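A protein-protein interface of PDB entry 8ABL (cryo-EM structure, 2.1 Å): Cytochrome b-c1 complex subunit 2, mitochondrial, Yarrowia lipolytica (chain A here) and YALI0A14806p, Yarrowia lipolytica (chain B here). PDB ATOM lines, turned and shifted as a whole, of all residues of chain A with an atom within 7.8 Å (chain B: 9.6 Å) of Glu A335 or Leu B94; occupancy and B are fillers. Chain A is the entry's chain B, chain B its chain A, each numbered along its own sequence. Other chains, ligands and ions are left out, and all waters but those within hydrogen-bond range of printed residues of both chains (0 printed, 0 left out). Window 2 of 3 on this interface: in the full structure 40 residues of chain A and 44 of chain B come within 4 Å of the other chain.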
ATOM      1  N   PHE A 262     -22.787  33.070  -7.086  1.00  0.00           N
ATOM      2  CA  PHE A 262     -21.432  32.705  -7.484  1.00  0.00           C
ATOM      3  C   PHE A 262     -20.541  32.459  -6.262  1.00  0.00           C
ATOM      4  O   PHE A 262     -19.979  31.365  -6.118  1.00  0.00           O
ATOM      5  CB  PHE A 262     -20.819  33.758  -8.415  1.00  0.00           C
ATOM      6  CG  PHE A 262     -19.316  33.714  -8.525  1.00  0.00           C
ATOM      7  CD1 PHE A 262     -18.664  32.597  -9.032  1.00  0.00           C
ATOM      8  CD2 PHE A 262     -18.552  34.783  -8.080  1.00  0.00           C
ATOM      9  CE1 PHE A 262     -17.277  32.553  -9.091  1.00  0.00           C
ATOM     10  CE2 PHE A 262     -17.168  34.736  -8.125  1.00  0.00           C
ATOM     11  CZ  PHE A 262     -16.534  33.620  -8.622  1.00  0.00           C
ATOM     12  N   SER A 268     -23.136  21.859  -2.720  1.00  0.00           N
ATOM     13  CA  SER A 268     -24.165  21.455  -3.671  1.00  0.00           C
ATOM     14  C   SER A 268     -24.536  19.979  -3.518  1.00  0.00           C
ATOM     15  O   SER A 268     -25.605  19.579  -3.980  1.00  0.00           O
ATOM     16  CB  SER A 268     -23.738  21.764  -5.065  1.00  0.00           C
ATOM     17  OG  SER A 268     -22.485  21.153  -5.345  1.00  0.00           O
ATOM     18  N   MET A 269     -23.677  19.190  -2.846  1.00  0.00           N
ATOM     19  CA  MET A 269     -23.907  17.761  -2.662  1.00  0.00           C
ATOM     20  C   MET A 269     -23.596  17.364  -1.220  1.00  0.00           C
ATOM     21  O   MET A 269     -22.823  18.042  -0.541  1.00  0.00           O
ATOM     22  CB  MET A 269     -23.035  16.874  -3.560  1.00  0.00           C
ATOM     23  CG  MET A 269     -22.665  17.438  -4.888  1.00  0.00           C
ATOM     24  SD  MET A 269     -20.931  17.894  -4.855  1.00  0.00           S
ATOM     25  CE  MET A 269     -20.159  16.282  -4.995  1.00  0.00           C
ATOM     26  N   GLY A 274     -17.871  22.051  -1.907  1.00  0.00           N
ATOM     27  CA  GLY A 274     -18.445  22.892  -2.945  1.00  0.00           C
ATOM     28  C   GLY A 274     -17.365  23.674  -3.688  1.00  0.00           C
ATOM     29  O   GLY A 274     -16.374  24.092  -3.086  1.00  0.00           O
ATOM     30  N   ALA A 275     -17.573  23.872  -4.995  1.00  0.00           N
ATOM     31  CA  ALA A 275     -16.591  24.480  -5.882  1.00  0.00           C
ATOM     32  C   ALA A 275     -16.553  26.005  -5.755  1.00  0.00           C
ATOM     33  O   ALA A 275     -15.625  26.633  -6.257  1.00  0.00           O
ATOM     34  CB  ALA A 275     -16.867  24.067  -7.303  1.00  0.00           C
ATOM     35  N   SER A 276     -17.547  26.573  -5.060  1.00  0.00           N
ATOM     36  CA  SER A 276     -17.705  28.008  -4.885  1.00  0.00           C
ATOM     37  C   SER A 276     -16.510  28.587  -4.124  1.00  0.00           C
ATOM     38  O   SER A 276     -15.989  27.932  -3.222  1.00  0.00           O
ATOM     39  CB  SER A 276     -19.003  28.308  -4.175  1.00  0.00           C
ATOM     40  OG  SER A 276     -18.771  28.684  -2.823  1.00  0.00           O
ATOM     41  N   GLN A 280     -14.588  27.115  -0.706  1.00  0.00           N
ATOM     42  CA  GLN A 280     -13.193  26.702  -0.744  1.00  0.00           C
ATOM     43  C   GLN A 280     -12.336  27.553   0.200  1.00  0.00           C
ATOM     44  O   GLN A 280     -11.108  27.525   0.104  1.00  0.00           O
ATOM     45  CB  GLN A 280     -12.637  26.768  -2.173  1.00  0.00           C
ATOM     46  CG  GLN A 280     -13.274  25.807  -3.169  1.00  0.00           C
ATOM     47  CD  GLN A 280     -12.855  24.361  -3.061  1.00  0.00           C
ATOM     48  OE1 GLN A 280     -11.835  23.993  -2.476  1.00  0.00           O
ATOM     49  NE2 GLN A 280     -13.622  23.517  -3.726  1.00  0.00           N
ATOM     50  N   VAL A 332     -13.410  37.413 -13.168  1.00  0.00           N
ATOM     51  CA  VAL A 332     -14.303  36.261 -13.175  1.00  0.00           C
ATOM     52  C   VAL A 332     -14.128  35.573 -14.530  1.00  0.00           C
ATOM     53  O   VAL A 332     -14.029  36.272 -15.532  1.00  0.00           O
ATOM     54  CB  VAL A 332     -15.771  36.696 -12.960  1.00  0.00           C
ATOM     55  CG1 VAL A 332     -16.551  35.685 -12.140  1.00  0.00           C
ATOM     56  CG2 VAL A 332     -15.940  38.090 -12.370  1.00  0.00           C
ATOM     57  N   THR A 333     -14.112  34.228 -14.582  1.00  0.00           N
ATOM     58  CA  THR A 333     -14.067  33.534 -15.864  1.00  0.00           C
ATOM     59  C   THR A 333     -15.473  33.444 -16.459  1.00  0.00           C
ATOM     60  O   THR A 333     -16.456  33.663 -15.754  1.00  0.00           O
ATOM     61  CB  THR A 333     -13.448  32.138 -15.741  1.00  0.00           C
ATOM     62  OG1 THR A 333     -14.452  31.163 -15.424  1.00  0.00           O
ATOM     63  CG2 THR A 333     -12.317  32.085 -14.737  1.00  0.00           C
ATOM     64  N   GLU A 334     -15.559  33.133 -17.758  1.00  0.00           N
ATOM     65  CA  GLU A 334     -16.835  32.949 -18.444  1.00  0.00           C
ATOM     66  C   GLU A 334     -17.616  31.785 -17.825  1.00  0.00           C
ATOM     67  O   GLU A 334     -18.835  31.882 -17.644  1.00  0.00           O
ATOM     68  CB  GLU A 334     -16.628  32.788 -19.954  1.00  0.00           C
ATOM     69  CG  GLU A 334     -17.917  32.860 -20.760  1.00  0.00           C
ATOM     70  CD  GLU A 334     -18.762  34.110 -20.565  1.00  0.00           C
ATOM     71  OE1 GLU A 334     -18.319  35.202 -20.994  1.00  0.00           O
ATOM     72  OE2 GLU A 334     -19.850  34.000 -19.957  1.00  0.00           O
ATOM     73  N   GLU A 335     -16.894  30.705 -17.474  1.00  0.00           N
ATOM     74  CA  GLU A 335     -17.472  29.547 -16.808  1.00  0.00           C
ATOM     75  C   GLU A 335     -18.069  29.987 -15.473  1.00  0.00           C
ATOM     76  O   GLU A 335     -19.171  29.568 -15.140  1.00  0.00           O
ATOM     77  CB  GLU A 335     -16.418  28.442 -16.653  1.00  0.00           C
ATOM     78  CG  GLU A 335     -16.888  27.183 -15.918  1.00  0.00           C
ATOM     79  CD  GLU A 335     -16.600  27.114 -14.420  1.00  0.00           C
ATOM     80  OE1 GLU A 335     -15.730  27.891 -13.954  1.00  0.00           O
ATOM     81  OE2 GLU A 335     -17.245  26.307 -13.712  1.00  0.00           O
ATOM     82  N   GLN A 336     -17.350  30.844 -14.734  1.00  0.00           N
ATOM     83  CA  GLN A 336     -17.781  31.262 -13.411  1.00  0.00           C
ATOM     84  C   GLN A 336     -19.030  32.122 -13.556  1.00  0.00           C
ATOM     85  O   GLN A 336     -19.922  32.047 -12.718  1.00  0.00           O
ATOM     86  CB  GLN A 336     -16.687  32.024 -12.667  1.00  0.00           C
ATOM     87  CG  GLN A 336     -15.552  31.148 -12.182  1.00  0.00           C
ATOM     88  CD  GLN A 336     -14.511  31.941 -11.435  1.00  0.00           C
ATOM     89  OE1 GLN A 336     -14.148  33.062 -11.802  1.00  0.00           O
ATOM     90  NE2 GLN A 336     -13.980  31.315 -10.400  1.00  0.00           N
ATOM     91  N   ALA A 337     -19.071  32.930 -14.620  1.00  0.00           N
ATOM     92  CA  ALA A 337     -20.205  33.802 -14.862  1.00  0.00           C
ATOM     93  C   ALA A 337     -21.430  32.969 -15.228  1.00  0.00           C
ATOM     94  O   ALA A 337     -22.530  33.332 -14.825  1.00  0.00           O
ATOM     95  CB  ALA A 337     -19.890  34.852 -15.899  1.00  0.00           C
ATOM     96  N   ALA A 338     -21.221  31.860 -15.951  1.00  0.00           N
ATOM     97  CA  ALA A 338     -22.322  30.998 -16.363  1.00  0.00           C
ATOM     98  C   ALA A 338     -22.876  30.222 -15.172  1.00  0.00           C
ATOM     99  O   ALA A 338     -24.085  30.113 -14.990  1.00  0.00           O
ATOM    100  CB  ALA A 338     -21.882  30.079 -17.478  1.00  0.00           C
ATOM    101  N   ARG A 339     -21.963  29.717 -14.342  1.00  0.00           N
ATOM    102  CA  ARG A 339     -22.290  29.095 -13.077  1.00  0.00           C
ATOM    103  C   ARG A 339     -23.070  30.061 -12.176  1.00  0.00           C
ATOM    104  O   ARG A 339     -23.859  29.574 -11.380  1.00  0.00           O
ATOM    105  CB  ARG A 339     -20.968  28.576 -12.505  1.00  0.00           C
ATOM    106  CG  ARG A 339     -21.058  27.792 -11.212  1.00  0.00           C
ATOM    107  CD  ARG A 339     -19.838  26.861 -11.137  1.00  0.00           C
ATOM    108  NE  ARG A 339     -18.460  27.339 -11.313  1.00  0.00           N
ATOM    109  CZ  ARG A 339     -17.678  27.779 -10.325  1.00  0.00           C
ATOM    110  NH1 ARG A 339     -18.154  27.846  -9.093  1.00  0.00           N
ATOM    111  NH2 ARG A 339     -16.448  28.191 -10.578  1.00  0.00           N
ATOM    112  N   ALA A 340     -22.802  31.385 -12.227  1.00  0.00           N
ATOM    113  CA  ALA A 340     -23.481  32.344 -11.363  1.00  0.00           C
ATOM    114  C   ALA A 340     -24.914  32.486 -11.853  1.00  0.00           C
ATOM    115  O   ALA A 340     -25.837  32.672 -11.064  1.00  0.00           O
ATOM    116  CB  ALA A 340     -22.805  33.708 -11.316  1.00  0.00           C
ATOM    117  N   TYR A 341     -25.078  32.480 -13.175  1.00  0.00           N
ATOM    118  CA  TYR A 341     -26.380  32.631 -13.789  1.00  0.00           C
ATOM    119  C   TYR A 341     -27.247  31.421 -13.463  1.00  0.00           C
ATOM    120  O   TYR A 341     -28.414  31.585 -13.142  1.00  0.00           O
ATOM    121  CB  TYR A 341     -26.214  32.723 -15.303  1.00  0.00           C
ATOM    122  CG  TYR A 341     -27.498  32.598 -16.069  1.00  0.00           C
ATOM    123  CD1 TYR A 341     -28.505  33.540 -15.926  1.00  0.00           C
ATOM    124  CD2 TYR A 341     -27.686  31.563 -16.968  1.00  0.00           C
ATOM    125  CE1 TYR A 341     -29.673  33.456 -16.662  1.00  0.00           C
ATOM    126  CE2 TYR A 341     -28.860  31.453 -17.696  1.00  0.00           C
ATOM    127  CZ  TYR A 341     -29.856  32.404 -17.542  1.00  0.00           C
ATOM    128  OH  TYR A 341     -31.021  32.328 -18.247  1.00  0.00           O
ATOM    129  N   ALA A 342     -26.645  30.225 -13.546  1.00  0.00           N
ATOM    130  CA  ALA A 342     -27.342  28.971 -13.330  1.00  0.00           C
ATOM    131  C   ALA A 342     -27.796  28.894 -11.879  1.00  0.00           C
ATOM    132  O   ALA A 342     -28.961  28.586 -11.642  1.00  0.00           O
ATOM    133  CB  ALA A 342     -26.481  27.788 -13.694  1.00  0.00           C
ATOM    134  N   LYS A 380     -28.556  37.329 -17.397  1.00  0.00           N
ATOM    135  CA  LYS A 380     -27.216  36.768 -17.380  1.00  0.00           C
ATOM    136  C   LYS A 380     -26.208  37.914 -17.353  1.00  0.00           C
ATOM    137  O   LYS A 380     -26.175  38.740 -18.266  1.00  0.00           O
ATOM    138  CB  LYS A 380     -26.967  35.825 -18.561  1.00  0.00           C
ATOM    139  CG  LYS A 380     -25.833  34.838 -18.307  1.00  0.00           C
ATOM    140  CD  LYS A 380     -25.383  33.995 -19.486  1.00  0.00           C
ATOM    141  CE  LYS A 380     -23.930  33.557 -19.394  1.00  0.00           C
ATOM    142  NZ  LYS A 380     -23.013  34.695 -19.128  1.00  0.00           N
ATOM    143  N   PRO A 383     -18.887  38.188 -17.213  1.00  0.00           N
ATOM    144  CA  PRO A 383     -17.785  38.235 -16.247  1.00  0.00           C
ATOM    145  C   PRO A 383     -17.411  39.666 -15.869  1.00  0.00           C
ATOM    146  O   PRO A 383     -17.243  39.958 -14.688  1.00  0.00           O
ATOM    147  CB  PRO A 383     -16.620  37.550 -16.968  1.00  0.00           C
ATOM    148  CG  PRO A 383     -17.293  36.656 -17.995  1.00  0.00           C
ATOM    149  CD  PRO A 383     -18.581  37.346 -18.377  1.00  0.00           C
ATOM    150  N   PHE B  81     -20.351  10.310  -3.400  1.00  0.00           N
ATOM    151  CA  PHE B  81     -20.048  11.668  -3.815  1.00  0.00           C
ATOM    152  C   PHE B  81     -18.550  11.946  -3.778  1.00  0.00           C
ATOM    153  O   PHE B  81     -18.144  13.096  -3.723  1.00  0.00           O
ATOM    154  CB  PHE B  81     -20.870  12.653  -2.986  1.00  0.00           C
ATOM    155  CG  PHE B  81     -22.355  12.407  -3.078  1.00  0.00           C
ATOM    156  CD1 PHE B  81     -23.072  12.853  -4.179  1.00  0.00           C
ATOM    157  CD2 PHE B  81     -23.031  11.697  -2.089  1.00  0.00           C
ATOM    158  CE1 PHE B  81     -24.442  12.648  -4.260  1.00  0.00           C
ATOM    159  CE2 PHE B  81     -24.398  11.476  -2.183  1.00  0.00           C
ATOM    160  CZ  PHE B  81     -25.100  11.944  -3.272  1.00  0.00           C
ATOM    161  N   ARG B  87     -15.679  11.171 -13.787  1.00  0.00           N
ATOM    162  CA  ARG B  87     -15.495  12.428 -13.081  1.00  0.00           C
ATOM    163  C   ARG B  87     -14.828  12.153 -11.740  1.00  0.00           C
ATOM    164  O   ARG B  87     -15.204  11.212 -11.062  1.00  0.00           O
ATOM    165  CB  ARG B  87     -16.835  13.138 -12.878  1.00  0.00           C
ATOM    166  CG  ARG B  87     -18.021  12.329 -13.389  1.00  0.00           C
ATOM    167  CD  ARG B  87     -19.266  12.991 -12.872  1.00  0.00           C
ATOM    168  NE  ARG B  87     -19.876  13.881 -13.852  1.00  0.00           N
ATOM    169  CZ  ARG B  87     -20.833  13.557 -14.718  1.00  0.00           C
ATOM    170  NH1 ARG B  87     -21.337  12.337 -14.729  1.00  0.00           N
ATOM    171  NH2 ARG B  87     -21.292  14.479 -15.543  1.00  0.00           N
ATOM    172  N   SER B  88     -13.832  12.968 -11.379  1.00  0.00           N
ATOM    173  CA  SER B  88     -13.222  12.918 -10.058  1.00  0.00           C
ATOM    174  C   SER B  88     -14.134  13.645  -9.071  1.00  0.00           C
ATOM    175  O   SER B  88     -15.174  14.161  -9.464  1.00  0.00           O
ATOM    176  CB  SER B  88     -11.865  13.557 -10.105  1.00  0.00           C
ATOM    177  OG  SER B  88     -11.988  14.971 -10.203  1.00  0.00           O
ATOM    178  N   GLN B  89     -13.731  13.716  -7.798  1.00  0.00           N
ATOM    179  CA  GLN B  89     -14.517  14.420  -6.792  1.00  0.00           C
ATOM    180  C   GLN B  89     -14.708  15.884  -7.193  1.00  0.00           C
ATOM    181  O   GLN B  89     -15.812  16.421  -7.080  1.00  0.00           O
ATOM    182  CB  GLN B  89     -13.860  14.310  -5.417  1.00  0.00           C
ATOM    183  CG  GLN B  89     -14.836  14.397  -4.261  1.00  0.00           C
ATOM    184  CD  GLN B  89     -14.999  15.766  -3.657  1.00  0.00           C
ATOM    185  OE1 GLN B  89     -14.163  16.654  -3.824  1.00  0.00           O
ATOM    186  NE2 GLN B  89     -16.086  15.940  -2.932  1.00  0.00           N
ATOM    187  N   HIS B  90     -13.621  16.504  -7.673  1.00  0.00           N
ATOM    188  CA  HIS B  90     -13.621  17.904  -8.055  1.00  0.00           C
ATOM    189  C   HIS B  90     -14.507  18.140  -9.271  1.00  0.00           C
ATOM    190  O   HIS B  90     -15.291  19.092  -9.306  1.00  0.00           O
ATOM    191  CB  HIS B  90     -12.200  18.435  -8.290  1.00  0.00           C
ATOM    192  CG  HIS B  90     -12.179  19.923  -8.253  1.00  0.00           C
ATOM    193  ND1 HIS B  90     -12.846  20.622  -7.265  1.00  0.00           N
ATOM    194  CD2 HIS B  90     -11.584  20.846  -9.040  1.00  0.00           C
ATOM    195  CE1 HIS B  90     -12.647  21.911  -7.421  1.00  0.00           C
ATOM    196  NE2 HIS B  90     -11.887  22.078  -8.518  1.00  0.00           N
ATOM    197  N   GLN B  91     -14.371  17.257 -10.267  1.00  0.00           N
ATOM    198  CA  GLN B  91     -15.181  17.339 -11.470  1.00  0.00           C
ATOM    199  C   GLN B  91     -16.658  17.168 -11.118  1.00  0.00           C
ATOM    200  O   GLN B  91     -17.484  17.920 -11.617  1.00  0.00           O
ATOM    201  CB  GLN B  91     -14.705  16.354 -12.540  1.00  0.00           C
ATOM    202  CG  GLN B  91     -15.218  16.680 -13.933  1.00  0.00           C
ATOM    203  CD  GLN B  91     -15.078  18.142 -14.283  1.00  0.00           C
ATOM    204  OE1 GLN B  91     -13.977  18.684 -14.358  1.00  0.00           O
ATOM    205  NE2 GLN B  91     -16.209  18.793 -14.501  1.00  0.00           N
ATOM    206  N   LEU B  92     -16.971  16.203 -10.241  1.00  0.00           N
ATOM    207  CA  LEU B  92     -18.329  15.976  -9.767  1.00  0.00           C
ATOM    208  C   LEU B  92     -18.904  17.263  -9.171  1.00  0.00           C
ATOM    209  O   LEU B  92     -19.965  17.718  -9.618  1.00  0.00           O
ATOM    210  CB  LEU B  92     -18.321  14.809  -8.774  1.00  0.00           C
ATOM    211  CG  LEU B  92     -19.678  14.237  -8.363  1.00  0.00           C
ATOM    212  CD1 LEU B  92     -20.585  13.982  -9.563  1.00  0.00           C
ATOM    213  CD2 LEU B  92     -19.485  12.963  -7.559  1.00  0.00           C
ATOM    214  N   GLU B  93     -18.162  17.892  -8.241  1.00  0.00           N
ATOM    215  CA  GLU B  93     -18.558  19.164  -7.646  1.00  0.00           C
ATOM    216  C   GLU B  93     -18.883  20.189  -8.734  1.00  0.00           C
ATOM    217  O   GLU B  93     -19.962  20.780  -8.731  1.00  0.00           O
ATOM    218  CB  GLU B  93     -17.453  19.716  -6.746  1.00  0.00           C
ATOM    219  CG  GLU B  93     -17.538  19.259  -5.305  1.00  0.00           C
ATOM    220  CD  GLU B  93     -16.239  19.379  -4.524  1.00  0.00           C
ATOM    221  OE1 GLU B  93     -15.178  19.654  -5.142  1.00  0.00           O
ATOM    222  OE2 GLU B  93     -16.276  19.150  -3.291  1.00  0.00           O
ATOM    223  N   LEU B  94     -17.950  20.348  -9.685  1.00  0.00           N
ATOM    224  CA  LEU B  94     -18.103  21.339 -10.736  1.00  0.00           C
ATOM    225  C   LEU B  94     -19.355  21.073 -11.564  1.00  0.00           C
ATOM    226  O   LEU B  94     -20.109  22.002 -11.848  1.00  0.00           O
ATOM    227  CB  LEU B  94     -16.854  21.370 -11.617  1.00  0.00           C
ATOM    228  CG  LEU B  94     -16.110  22.698 -11.611  1.00  0.00           C
ATOM    229  CD1 LEU B  94     -14.870  22.597 -10.748  1.00  0.00           C
ATOM    230  CD2 LEU B  94     -15.728  23.094 -13.028  1.00  0.00           C
ATOM    231  N   ASP B  95     -19.575  19.805 -11.926  1.00  0.00           N
ATOM    232  CA  ASP B  95     -20.692  19.428 -12.775  1.00  0.00           C
ATOM    233  C   ASP B  95     -22.028  19.837 -12.159  1.00  0.00           C
ATOM    234  O   ASP B  95     -22.876  20.395 -12.850  1.00  0.00           O
ATOM    235  CB  ASP B  95     -20.617  17.945 -13.130  1.00  0.00           C
ATOM    236  CG  ASP B  95     -19.516  17.638 -14.128  1.00  0.00           C
ATOM    237  OD1 ASP B  95     -19.302  18.467 -15.044  1.00  0.00           O
ATOM    238  OD2 ASP B  95     -18.903  16.558 -14.004  1.00  0.00           O
ATOM    239  N   ILE B  96     -22.193  19.571 -10.855  1.00  0.00           N
ATOM    240  CA  ILE B  96     -23.425  19.896 -10.152  1.00  0.00           C
ATOM    241  C   ILE B  96     -23.581  21.405 -10.007  1.00  0.00           C
ATOM    242  O   ILE B  96     -24.679  21.927 -10.191  1.00  0.00           O
ATOM    243  CB  ILE B  96     -23.514  19.124  -8.824  1.00  0.00           C
ATOM    244  CG1 ILE B  96     -23.635  17.635  -9.158  1.00  0.00           C
ATOM    245  CG2 ILE B  96     -24.687  19.590  -7.960  1.00  0.00           C
ATOM    246  CD1 ILE B  96     -22.971  16.726  -8.180  1.00  0.00           C
ATOM    247  N   GLU B  97     -22.480  22.092  -9.674  1.00  0.00           N
ATOM    248  CA  GLU B  97     -22.465  23.544  -9.568  1.00  0.00           C
ATOM    249  C   GLU B  97     -22.866  24.177 -10.903  1.00  0.00           C
ATOM    250  O   GLU B  97     -23.602  25.163 -10.909  1.00  0.00           O
ATOM    251  CB  GLU B  97     -21.097  24.039  -9.093  1.00  0.00           C
ATOM    252  CG  GLU B  97     -21.157  24.921  -7.859  1.00  0.00           C
ATOM    253  CD  GLU B  97     -20.829  24.241  -6.536  1.00  0.00           C
ATOM    254  OE1 GLU B  97     -20.990  24.899  -5.486  1.00  0.00           O
ATOM    255  OE2 GLU B  97     -20.408  23.062  -6.551  1.00  0.00           O
ATOM    256  N   ASN B  98     -22.434  23.564 -12.017  1.00  0.00           N
ATOM    257  CA  ASN B  98     -22.718  24.093 -13.342  1.00  0.00           C
ATOM    258  C   ASN B  98     -24.186  23.884 -13.710  1.00  0.00           C
ATOM    259  O   ASN B  98     -24.757  24.691 -14.440  1.00  0.00           O
ATOM    260  CB  ASN B  98     -21.748  23.575 -14.407  1.00  0.00           C
ATOM    261  CG  ASN B  98     -20.437  24.333 -14.434  1.00  0.00           C
ATOM    262  OD1 ASN B  98     -20.404  25.524 -14.741  1.00  0.00           O
ATOM    263  ND2 ASN B  98     -19.349  23.649 -14.122  1.00  0.00           N
ATOM    264  N   MET B  99     -24.783  22.792 -13.220  1.00  0.00           N
ATOM    265  CA  MET B  99     -26.193  22.510 -13.436  1.00  0.00           C
ATOM    266  C   MET B  99     -27.034  23.581 -12.743  1.00  0.00           C
ATOM    267  O   MET B  99     -28.007  24.055 -13.324  1.00  0.00           O
ATOM    268  CB  MET B  99     -26.512  21.123 -12.877  1.00  0.00           C
ATOM    269  CG  MET B  99     -27.957  20.730 -12.884  1.00  0.00           C
ATOM    270  SD  MET B  99     -28.183  19.135 -12.067  1.00  0.00           S
ATOM    271  CE  MET B  99     -28.001  19.591 -10.341  1.00  0.00           C
ATOM    272  N   GLY B 100     -26.635  23.958 -11.520  1.00  0.00           N
ATOM    273  CA  GLY B 100     -27.264  25.068 -10.819  1.00  0.00           C
ATOM    274  C   GLY B 100     -28.117  24.630  -9.634  1.00  0.00           C
ATOM    275  O   GLY B 100     -28.343  25.415  -8.714  1.00  0.00           O
ATOM    276  N   GLY B 101     -28.584  23.376  -9.654  1.00  0.00           N
ATOM    277  CA  GLY B 101     -29.363  22.849  -8.546  1.00  0.00           C
ATOM    278  C   GLY B 101     -28.460  22.145  -7.539  1.00  0.00           C
ATOM    279  O   GLY B 101     -27.263  22.438  -7.471  1.00  0.00           O
ATOM    280  N   LYS B 125     -29.133  16.176 -17.429  1.00  0.00           N
ATOM    281  CA  LYS B 125     -27.804  16.217 -16.830  1.00  0.00           C
ATOM    282  C   LYS B 125     -27.826  15.487 -15.487  1.00  0.00           C
ATOM    283  O   LYS B 125     -26.934  14.716 -15.161  1.00  0.00           O
ATOM    284  CB  LYS B 125     -27.340  17.651 -16.574  1.00  0.00           C
ATOM    285  CG  LYS B 125     -27.331  18.583 -17.774  1.00  0.00           C
ATOM    286  CD  LYS B 125     -26.972  19.987 -17.351  1.00  0.00           C
ATOM    287  CE  LYS B 125     -26.835  20.945 -18.514  1.00  0.00           C
ATOM    288  NZ  LYS B 125     -28.025  20.871 -19.391  1.00  0.00           N
ATOM    289  N   ILE B 129     -25.840  12.257 -13.963  1.00  0.00           N
ATOM    290  CA  ILE B 129     -24.982  12.255 -12.787  1.00  0.00           C
ATOM    291  C   ILE B 129     -25.409  11.187 -11.784  1.00  0.00           C
ATOM    292  O   ILE B 129     -24.555  10.505 -11.237  1.00  0.00           O
ATOM    293  CB  ILE B 129     -24.910  13.660 -12.184  1.00  0.00           C
ATOM    294  CG1 ILE B 129     -24.103  14.569 -13.110  1.00  0.00           C
ATOM    295  CG2 ILE B 129     -24.358  13.645 -10.767  1.00  0.00           C
ATOM    296  CD1 ILE B 129     -24.383  16.031 -12.895  1.00  0.00           C
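O of Gly A274 sits at hydrogen-bond distance from NE2 of Gln A280 (2.9 Å). N of Glu A335 is in hydrogen-bond range of OG1 of Thr A333, at 3.2 Å. NE of Arg A339 lies within salt-bridge range of OE2 of Glu A335 (2.9 Å). The side-chain carboxylate of Glu B93 lies within hydrogen-bond range of a ring nitrogen (ND1) of His B90. The side-chain carboxylate (OE2) of Glu B93 sits at hydrogen-bond distance from the side-chain amide nitrogen (NE2) of Gln B89 (3.2 Å). OG of Ser A268 lies within hydrogen-bond range of SD of Met A269.
Hydrophobic or aromatic side chains of chain A within 4 Å of the printed part of chain B: Met A269, Ala A275 and Ala A342. Among the printed residues, no Asp or Glu carboxylate lies within 4 Å of a Lys or Arg side-chain nitrogen of the other chain.
The side-chain carboxylate (OE2) of Glu B97 lies within hydrogen-bond range of the side-chain hydroxyl (OG) of Ser A268 (3.1 Å). The side-chain carboxylate (OE2) of Glu A335 lies close to the side-chain amide oxygen (OD1) of Asn B98 (3.4 Å). The backbone NH (N) of Ala A275 lies within hydrogen-bond range of the side-chain carboxylate (OE2) of Glu B97.
Among the printed residues, merely in contact across the chains: Ser A268 with Ile B96 (3.7 Å), Met A269 with Phe B81 (3.98 Å), Met A269 with Leu B92 (3.97 Å), Met A269 with Glu B93 (3.7 Å), Met A269 with Ile B96 (3.4 Å), Gly A274 with Glu B93 (3.6 Å), Ser A276 with Glu B97 (3.9 Å), Glu A335 with Leu B94 (3.6 Å), Arg A339 with Glu B97 (3.7 Å), Arg A339 with Asn B98 (3.8 Å), Ala A342 with Asn B98 (3.6 Å) and Ala A342 with Gly B100 (3.99 Å).
Of the printed residues of chain B, Gly A274 touches Glu B93 (3.6 Å). No residue of chain B comes within 4 Å of Thr A333. Printed residues of chain B within 4 Å of Glu A335: Leu B94 and Asn B98. No residue of chain B comes within 4 Å of Ala A337. No residue of chain B comes within 4 Å of Ala A338. Of the printed residues of chain A, Leu B92 touches Met A269. The nearest residue of chain B that does not touch Glu A335 is Glu B97 (6.4 Å).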
